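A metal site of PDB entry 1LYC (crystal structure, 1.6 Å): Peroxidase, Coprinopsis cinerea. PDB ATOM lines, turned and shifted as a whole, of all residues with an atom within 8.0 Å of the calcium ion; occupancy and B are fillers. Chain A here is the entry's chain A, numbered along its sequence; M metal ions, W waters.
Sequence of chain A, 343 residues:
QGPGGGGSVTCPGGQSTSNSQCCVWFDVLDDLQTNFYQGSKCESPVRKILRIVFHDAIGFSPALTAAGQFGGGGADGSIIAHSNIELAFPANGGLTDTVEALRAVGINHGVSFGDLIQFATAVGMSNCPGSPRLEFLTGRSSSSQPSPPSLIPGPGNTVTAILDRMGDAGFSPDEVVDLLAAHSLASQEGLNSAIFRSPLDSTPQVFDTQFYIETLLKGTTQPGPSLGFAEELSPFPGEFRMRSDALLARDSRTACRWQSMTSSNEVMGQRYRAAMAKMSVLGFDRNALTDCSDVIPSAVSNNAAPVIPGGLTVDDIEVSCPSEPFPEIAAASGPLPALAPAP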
ATOM      1  N   ILE A  52      16.153  21.303 -24.092  1.00  0.00           N
ATOM      2  CA  ILE A  52      14.795  21.485 -24.576  1.00  0.00           C
ATOM      3  C   ILE A  52      13.765  20.621 -23.837  1.00  0.00           C
ATOM      4  O   ILE A  52      12.703  21.125 -23.453  1.00  0.00           O
ATOM      5  CB  ILE A  52      14.731  21.200 -26.110  1.00  0.00           C
ATOM      6  CG1 ILE A  52      15.441  22.347 -26.848  1.00  0.00           C
ATOM      7  CG2 ILE A  52      13.292  21.044 -26.592  1.00  0.00           C
ATOM      8  CD1 ILE A  52      15.611  22.131 -28.325  1.00  0.00           C
ATOM      9  N   VAL A  53      14.076  19.345 -23.645  1.00  0.00           N
ATOM     10  CA  VAL A  53      13.167  18.450 -22.951  1.00  0.00           C
ATOM     11  C   VAL A  53      12.960  18.887 -21.496  1.00  0.00           C
ATOM     12  O   VAL A  53      11.845  18.802 -20.976  1.00  0.00           O
ATOM     13  CB  VAL A  53      13.673  16.982 -22.993  1.00  0.00           C
ATOM     14  CG1 VAL A  53      14.957  16.820 -22.177  1.00  0.00           C
ATOM     15  CG2 VAL A  53      12.580  16.042 -22.502  1.00  0.00           C
ATOM     16  N   PHE A  54      14.017  19.356 -20.847  1.00  0.00           N
ATOM     17  CA  PHE A  54      13.898  19.841 -19.470  1.00  0.00           C
ATOM     18  C   PHE A  54      13.040  21.110 -19.444  1.00  0.00           C
ATOM     19  O   PHE A  54      12.067  21.202 -18.704  1.00  0.00           O
ATOM     20  CB  PHE A  54      15.280  20.133 -18.866  1.00  0.00           C
ATOM     21  CG  PHE A  54      15.225  20.799 -17.494  1.00  0.00           C
ATOM     22  CD1 PHE A  54      16.028  21.902 -17.206  1.00  0.00           C
ATOM     23  CD2 PHE A  54      14.374  20.309 -16.490  1.00  0.00           C
ATOM     24  CE1 PHE A  54      15.984  22.510 -15.941  1.00  0.00           C
ATOM     25  CE2 PHE A  54      14.330  20.917 -15.225  1.00  0.00           C
ATOM     26  CZ  PHE A  54      15.133  22.011 -14.957  1.00  0.00           C
ATOM     27  N   HIS A  55      13.419  22.083 -20.278  1.00  0.00           N
ATOM     28  CA  HIS A  55      12.734  23.373 -20.354  1.00  0.00           C
ATOM     29  C   HIS A  55      11.284  23.301 -20.820  1.00  0.00           C
ATOM     30  O   HIS A  55      10.476  24.161 -20.459  1.00  0.00           O
ATOM     31  CB  HIS A  55      13.512  24.337 -21.256  1.00  0.00           C
ATOM     32  CG  HIS A  55      14.830  24.761 -20.689  1.00  0.00           C
ATOM     33  ND1 HIS A  55      15.614  25.745 -21.267  1.00  0.00           N
ATOM     34  CD2 HIS A  55      15.504  24.360 -19.577  1.00  0.00           C
ATOM     35  CE1 HIS A  55      16.704  25.918 -20.541  1.00  0.00           C
ATOM     36  NE2 HIS A  55      16.657  25.100 -19.514  1.00  0.00           N
ATOM     37  N   ASP A  56      10.946  22.303 -21.623  1.00  0.00           N
ATOM     38  CA  ASP A  56       9.564  22.158 -22.089  1.00  0.00           C
ATOM     39  C   ASP A  56       8.713  21.563 -20.968  1.00  0.00           C
ATOM     40  O   ASP A  56       7.641  22.085 -20.647  1.00  0.00           O
ATOM     41  CB  ASP A  56       9.477  21.261 -23.331  1.00  0.00           C
ATOM     42  CG  ASP A  56       8.044  21.123 -23.850  1.00  0.00           C
ATOM     43  OD1 ASP A  56       7.327  22.153 -23.932  1.00  0.00           O
ATOM     44  OD2 ASP A  56       7.626  19.988 -24.193  1.00  0.00           O
ATOM     45  N   ALA A  57       9.197  20.490 -20.365  1.00  0.00           N
ATOM     46  CA  ALA A  57       8.468  19.809 -19.304  1.00  0.00           C
ATOM     47  C   ALA A  57       8.311  20.585 -17.996  1.00  0.00           C
ATOM     48  O   ALA A  57       7.257  20.507 -17.348  1.00  0.00           O
ATOM     49  CB  ALA A  57       9.125  18.455 -19.014  1.00  0.00           C
ATOM     50  N   ILE A  58       9.349  21.325 -17.613  1.00  0.00           N
ATOM     51  CA  ILE A  58       9.347  22.071 -16.344  1.00  0.00           C
ATOM     52  C   ILE A  58       8.349  23.237 -16.273  1.00  0.00           C
ATOM     53  O   ILE A  58       8.126  23.813 -15.211  1.00  0.00           O
ATOM     54  CB  ILE A  58      10.775  22.580 -16.008  1.00  0.00           C
ATOM     55  CG1 ILE A  58      10.873  22.871 -14.505  1.00  0.00           C
ATOM     56  CG2 ILE A  58      11.098  23.842 -16.798  1.00  0.00           C
ATOM     57  CD1 ILE A  58      10.642  21.664 -13.619  1.00  0.00           C
ATOM     58  N   GLY A  59       7.732  23.579 -17.409  1.00  0.00           N
ATOM     59  CA  GLY A  59       6.737  24.646 -17.396  1.00  0.00           C
ATOM     60  C   GLY A  59       5.451  24.012 -16.918  1.00  0.00           C
ATOM     61  O   GLY A  59       4.500  23.840 -17.698  1.00  0.00           O
ATOM     62  N   PHE A  60       5.433  23.656 -15.638  1.00  0.00           N
ATOM     63  CA  PHE A  60       4.319  22.978 -14.976  1.00  0.00           C
ATOM     64  C   PHE A  60       4.347  23.310 -13.485  1.00  0.00           C
ATOM     65  O   PHE A  60       5.263  22.899 -12.761  1.00  0.00           O
ATOM     66  CB  PHE A  60       4.481  21.465 -15.179  1.00  0.00           C
ATOM     67  CG  PHE A  60       3.435  20.637 -14.491  1.00  0.00           C
ATOM     68  CD1 PHE A  60       2.142  20.567 -14.986  1.00  0.00           C
ATOM     69  CD2 PHE A  60       3.768  19.883 -13.365  1.00  0.00           C
ATOM     70  CE1 PHE A  60       1.178  19.759 -14.358  1.00  0.00           C
ATOM     71  CE2 PHE A  60       2.815  19.078 -12.728  1.00  0.00           C
ATOM     72  CZ  PHE A  60       1.526  19.013 -13.230  1.00  0.00           C
ATOM     73  N   GLY A  72       0.827  25.797 -16.482  1.00  0.00           N
ATOM     74  CA  GLY A  72       1.671  25.265 -17.535  1.00  0.00           C
ATOM     75  C   GLY A  72       1.206  23.861 -17.885  1.00  0.00           C
ATOM     76  O   GLY A  72       0.594  23.183 -17.056  1.00  0.00           O
ATOM     77  N   GLY A  73       1.510  23.419 -19.102  1.00  0.00           N
ATOM     78  CA  GLY A  73       1.096  22.097 -19.541  1.00  0.00           C
ATOM     79  C   GLY A  73       2.117  20.981 -19.477  1.00  0.00           C
ATOM     80  O   GLY A  73       1.897  19.919 -20.061  1.00  0.00           O
ATOM     81  N   GLY A  74       3.221  21.216 -18.779  1.00  0.00           N
ATOM     82  CA  GLY A  74       4.251  20.192 -18.669  1.00  0.00           C
ATOM     83  C   GLY A  74       4.877  19.840 -19.998  1.00  0.00           C
ATOM     84  O   GLY A  74       5.194  20.727 -20.795  1.00  0.00           O
ATOM     85  N   ALA A  75       5.060  18.535 -20.254  1.00  0.00           N
ATOM     86  CA  ALA A  75       5.674  18.044 -21.487  1.00  0.00           C
ATOM     87  C   ALA A  75       4.740  18.087 -22.692  1.00  0.00           C
ATOM     88  O   ALA A  75       4.581  17.099 -23.420  1.00  0.00           O
ATOM     89  CB  ALA A  75       6.182  16.626 -21.267  1.00  0.00           C
ATOM     90  N   ASP A  76       4.137  19.252 -22.924  1.00  0.00           N
ATOM     91  CA  ASP A  76       3.189  19.450 -24.009  1.00  0.00           C
ATOM     92  C   ASP A  76       3.782  19.981 -25.307  1.00  0.00           C
ATOM     93  O   ASP A  76       3.043  20.257 -26.261  1.00  0.00           O
ATOM     94  CB  ASP A  76       2.072  20.371 -23.526  1.00  0.00           C
ATOM     95  CG  ASP A  76       2.578  21.756 -23.151  1.00  0.00           C
ATOM     96  OD1 ASP A  76       1.775  22.571 -22.667  1.00  0.00           O
ATOM     97  OD2 ASP A  76       3.785  22.017 -23.345  1.00  0.00           O
ATOM     98  N   GLY A  77       5.094  20.126 -25.371  1.00  0.00           N
ATOM     99  CA  GLY A  77       5.730  20.625 -26.584  1.00  0.00           C
ATOM    100  C   GLY A  77       5.495  22.095 -26.890  1.00  0.00           C
ATOM    101  O   GLY A  77       5.750  22.555 -28.017  1.00  0.00           O
ATOM    102  N   SER A  78       5.026  22.835 -25.897  1.00  0.00           N
ATOM    103  CA  SER A  78       4.760  24.272 -26.053  1.00  0.00           C
ATOM    104  C   SER A  78       6.007  25.095 -26.426  1.00  0.00           C
ATOM    105  O   SER A  78       5.894  26.170 -27.011  1.00  0.00           O
ATOM    106  CB  SER A  78       4.158  24.838 -24.770  1.00  0.00           C
ATOM    107  OG  SER A  78       5.040  24.649 -23.678  1.00  0.00           O
ATOM    108  N   ILE A  79       7.193  24.573 -26.080  1.00  0.00           N
ATOM    109  CA  ILE A  79       8.442  25.273 -26.378  1.00  0.00           C
ATOM    110  C   ILE A  79       8.649  25.353 -27.889  1.00  0.00           C
ATOM    111  O   ILE A  79       9.320  26.263 -28.383  1.00  0.00           O
ATOM    112  CB  ILE A  79       9.653  24.583 -25.684  1.00  0.00           C
ATOM    113  CG1 ILE A  79      10.896  25.483 -25.807  1.00  0.00           C
ATOM    114  CG2 ILE A  79       9.906  23.210 -26.295  1.00  0.00           C
ATOM    115  CD1 ILE A  79      12.111  24.974 -25.058  1.00  0.00           C
ATOM    116  N   ILE A  80       8.068  24.413 -28.616  1.00  0.00           N
ATOM    117  CA  ILE A  80       8.158  24.419 -30.074  1.00  0.00           C
ATOM    118  C   ILE A  80       6.877  25.090 -30.575  1.00  0.00           C
ATOM    119  O   ILE A  80       6.923  26.012 -31.399  1.00  0.00           O
ATOM    120  CB  ILE A  80       8.214  22.969 -30.683  1.00  0.00           C
ATOM    121  CG1 ILE A  80       9.407  22.194 -30.118  1.00  0.00           C
ATOM    122  CG2 ILE A  80       8.356  23.049 -32.207  1.00  0.00           C
ATOM    123  CD1 ILE A  80       9.485  20.758 -30.565  1.00  0.00           C
ATOM    124  N   HIS A  82       4.964  27.144 -29.129  1.00  0.00           N
ATOM    125  CA  HIS A  82       4.915  28.556 -28.753  1.00  0.00           C
ATOM    126  C   HIS A  82       6.324  29.091 -28.562  1.00  0.00           C
ATOM    127  O   HIS A  82       6.595  29.815 -27.603  1.00  0.00           O
ATOM    128  CB  HIS A  82       4.098  28.715 -27.477  1.00  0.00           C
ATOM    129  CG  HIS A  82       2.694  28.213 -27.584  1.00  0.00           C
ATOM    130  ND1 HIS A  82       1.715  28.893 -28.269  1.00  0.00           N
ATOM    131  CD2 HIS A  82       2.120  27.055 -27.176  1.00  0.00           C
ATOM    132  CE1 HIS A  82       0.596  28.186 -28.273  1.00  0.00           C
ATOM    133  NE2 HIS A  82       0.827  27.066 -27.609  1.00  0.00           N
ATOM    134  N   GLU A  86       8.244  31.444 -25.776  1.00  0.00           N
ATOM    135  CA  GLU A  86       9.198  30.712 -24.950  1.00  0.00           C
ATOM    136  C   GLU A  86      10.681  30.887 -25.276  1.00  0.00           C
ATOM    137  O   GLU A  86      11.509  30.968 -24.362  1.00  0.00           O
ATOM    138  CB  GLU A  86       8.806  29.235 -24.920  1.00  0.00           C
ATOM    139  CG  GLU A  86       7.501  29.001 -24.153  1.00  0.00           C
ATOM    140  CD  GLU A  86       7.229  27.558 -23.859  1.00  0.00           C
ATOM    141  OE1 GLU A  86       8.196  26.809 -23.565  1.00  0.00           O
ATOM    142  OE2 GLU A  86       6.040  27.167 -23.890  1.00  0.00           O
ATOM    143  N   GLY A 114       5.184  17.358 -28.215  1.00  0.00           N
ATOM    144  CA  GLY A 114       5.483  16.826 -26.902  1.00  0.00           C
ATOM    145  C   GLY A 114       6.071  15.419 -26.973  1.00  0.00           C
ATOM    146  O   GLY A 114       6.961  15.077 -26.199  1.00  0.00           O
ATOM    147  N   ILE A 117       9.821  15.583 -28.818  1.00  0.00           N
ATOM    148  CA  ILE A 117      10.883  16.030 -27.917  1.00  0.00           C
ATOM    149  C   ILE A 117      11.284  14.870 -27.013  1.00  0.00           C
ATOM    150  O   ILE A 117      12.477  14.572 -26.856  1.00  0.00           O
ATOM    151  CB  ILE A 117      10.425  17.231 -27.045  1.00  0.00           C
ATOM    152  CG1 ILE A 117      10.160  18.452 -27.918  1.00  0.00           C
ATOM    153  CG2 ILE A 117      11.498  17.560 -26.002  1.00  0.00           C
ATOM    154  CD1 ILE A 117       9.630  19.659 -27.154  1.00  0.00           C
ATOM    155  N   SER A 144      -1.147  22.724 -27.065  1.00  0.00           N
ATOM    156  CA  SER A 144      -0.494  23.249 -25.882  1.00  0.00           C
ATOM    157  C   SER A 144      -0.614  24.772 -25.870  1.00  0.00           C
ATOM    158  O   SER A 144      -0.889  25.393 -26.893  1.00  0.00           O
ATOM    159  CB  SER A 144       0.998  22.892 -25.894  1.00  0.00           C
ATOM    160  OG  SER A 144       1.702  23.759 -26.775  1.00  0.00           O
ATOM    161  N   GLN A 145      -0.395  25.358 -24.697  1.00  0.00           N
ATOM    162  CA  GLN A 145      -0.430  26.808 -24.535  1.00  0.00           C
ATOM    163  C   GLN A 145       0.972  27.214 -24.153  1.00  0.00           C
ATOM    164  O   GLN A 145       1.752  26.384 -23.673  1.00  0.00           O
ATOM    165  CB  GLN A 145      -1.409  27.203 -23.430  1.00  0.00           C
ATOM    166  CG  GLN A 145      -2.814  26.778 -23.744  1.00  0.00           C
ATOM    167  CD  GLN A 145      -3.811  27.471 -22.859  1.00  0.00           C
ATOM    168  OE1 GLN A 145      -3.766  27.333 -21.641  1.00  0.00           O
ATOM    169  NE2 GLN A 145      -4.712  28.235 -23.476  1.00  0.00           N
ATOM    170  N   PRO A 146       1.330  28.487 -24.342  1.00  0.00           N
ATOM    171  CA  PRO A 146       2.689  28.889 -23.975  1.00  0.00           C
ATOM    172  C   PRO A 146       2.918  28.715 -22.477  1.00  0.00           C
ATOM    173  O   PRO A 146       1.993  28.872 -21.671  1.00  0.00           O
ATOM    174  CB  PRO A 146       2.755  30.339 -24.433  1.00  0.00           C
ATOM    175  CG  PRO A 146       1.333  30.803 -24.271  1.00  0.00           C
ATOM    176  CD  PRO A 146       0.545  29.642 -24.817  1.00  0.00           C
ATOM    177  N   SER A 147       4.142  28.356 -22.110  1.00  0.00           N
ATOM    178  CA  SER A 147       4.486  28.161 -20.697  1.00  0.00           C
ATOM    179  C   SER A 147       4.545  29.483 -19.932  1.00  0.00           C
ATOM    180  O   SER A 147       4.917  30.520 -20.486  1.00  0.00           O
ATOM    181  CB  SER A 147       5.843  27.451 -20.568  1.00  0.00           C
ATOM    182  OG  SER A 147       6.264  27.374 -19.200  1.00  0.00           O
ATOM    183  N   PRO A 148       4.159  29.456 -18.643  1.00  0.00           N
ATOM    184  CA  PRO A 148       4.213  30.687 -17.853  1.00  0.00           C
ATOM    185  C   PRO A 148       5.709  31.036 -17.721  1.00  0.00           C
ATOM    186  O   PRO A 148       6.553  30.139 -17.670  1.00  0.00           O
ATOM    187  CB  PRO A 148       3.611  30.257 -16.512  1.00  0.00           C
ATOM    188  CG  PRO A 148       2.673  29.176 -16.894  1.00  0.00           C
ATOM    189  CD  PRO A 148       3.447  28.397 -17.911  1.00  0.00           C
ATOM    190  N   LEU A 282       4.777  14.990 -17.049  1.00  0.00           N
ATOM    191  CA  LEU A 282       4.319  16.080 -16.204  1.00  0.00           C
ATOM    192  C   LEU A 282       3.188  16.728 -16.979  1.00  0.00           C
ATOM    193  O   LEU A 282       3.361  17.148 -18.130  1.00  0.00           O
ATOM    194  CB  LEU A 282       5.430  17.102 -15.941  1.00  0.00           C
ATOM    195  CG  LEU A 282       6.548  16.762 -14.943  1.00  0.00           C
ATOM    196  CD1 LEU A 282       7.453  17.975 -14.759  1.00  0.00           C
ATOM    197  CD2 LEU A 282       5.947  16.362 -13.592  1.00  0.00           C
ATOM    198  N   PHE A 284       0.436  15.025 -17.558  1.00  0.00           N
ATOM    199  CA  PHE A 284      -0.172  13.895 -18.263  1.00  0.00           C
ATOM    200  C   PHE A 284      -0.447  12.702 -17.351  1.00  0.00           C
ATOM    201  O   PHE A 284       0.118  12.589 -16.256  1.00  0.00           O
ATOM    202  CB  PHE A 284       0.731  13.441 -19.403  1.00  0.00           C
ATOM    203  CG  PHE A 284       0.873  14.446 -20.496  1.00  0.00           C
ATOM    204  CD1 PHE A 284      -0.075  14.513 -21.512  1.00  0.00           C
ATOM    205  CD2 PHE A 284       1.937  15.336 -20.514  1.00  0.00           C
ATOM    206  CE1 PHE A 284       0.032  15.460 -22.531  1.00  0.00           C
ATOM    207  CE2 PHE A 284       2.054  16.286 -21.524  1.00  0.00           C
ATOM    208  CZ  PHE A 284       1.106  16.353 -22.540  1.00  0.00           C
HETATM  209 CA    CA M   1       5.963  22.640 -22.034  1.00  0.00          CA
HETATM  210  O   HOH W   1       7.782  24.925 -22.060  1.00  0.00           O
HETATM  211  O   HOH W   2       4.867  24.114 -20.107  1.00  0.00           O
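The backbone NH (N) of Gly 74 lies within hydrogen-bond range of the backbone carbonyl oxygen (O) of Gly 59 (3.1 Å). The side-chain carboxylate (OD2) of Asp 56 is in hydrogen-bond range of the backbone NH (N) of Gly 77 (2.8 Å). OD1 of Asp 56 sits close to N of Ile 79, 3.2 Å away. OG of Ser 78 sits close to OE2 of Glu 86.
Within 4 Å of the calcium ion: Asp 56, Gly 74, Asp 76 and Ser 78.
O of Asp 56 binds the calcium ion, 2.2 Å away. The calcium ion is bound by OD1 of Asp 56, at 2.4 Å. O of Gly 74 binds the calcium ion (2.4 Å). OD2 of Asp 76 binds the calcium ion. Water W2 binds the calcium ion, 2.7 Å away. The side-chain hydroxyl (OG) of Ser 78 is bound to the calcium ion (2.8 Å). Slightly farther from the calcium ion lies water W1 (2.9 Å).
Water W1 lies within hydrogen-bond range of OE1 of Glu 86 (2.4 Å) and O of His 55 (3.2 Å).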
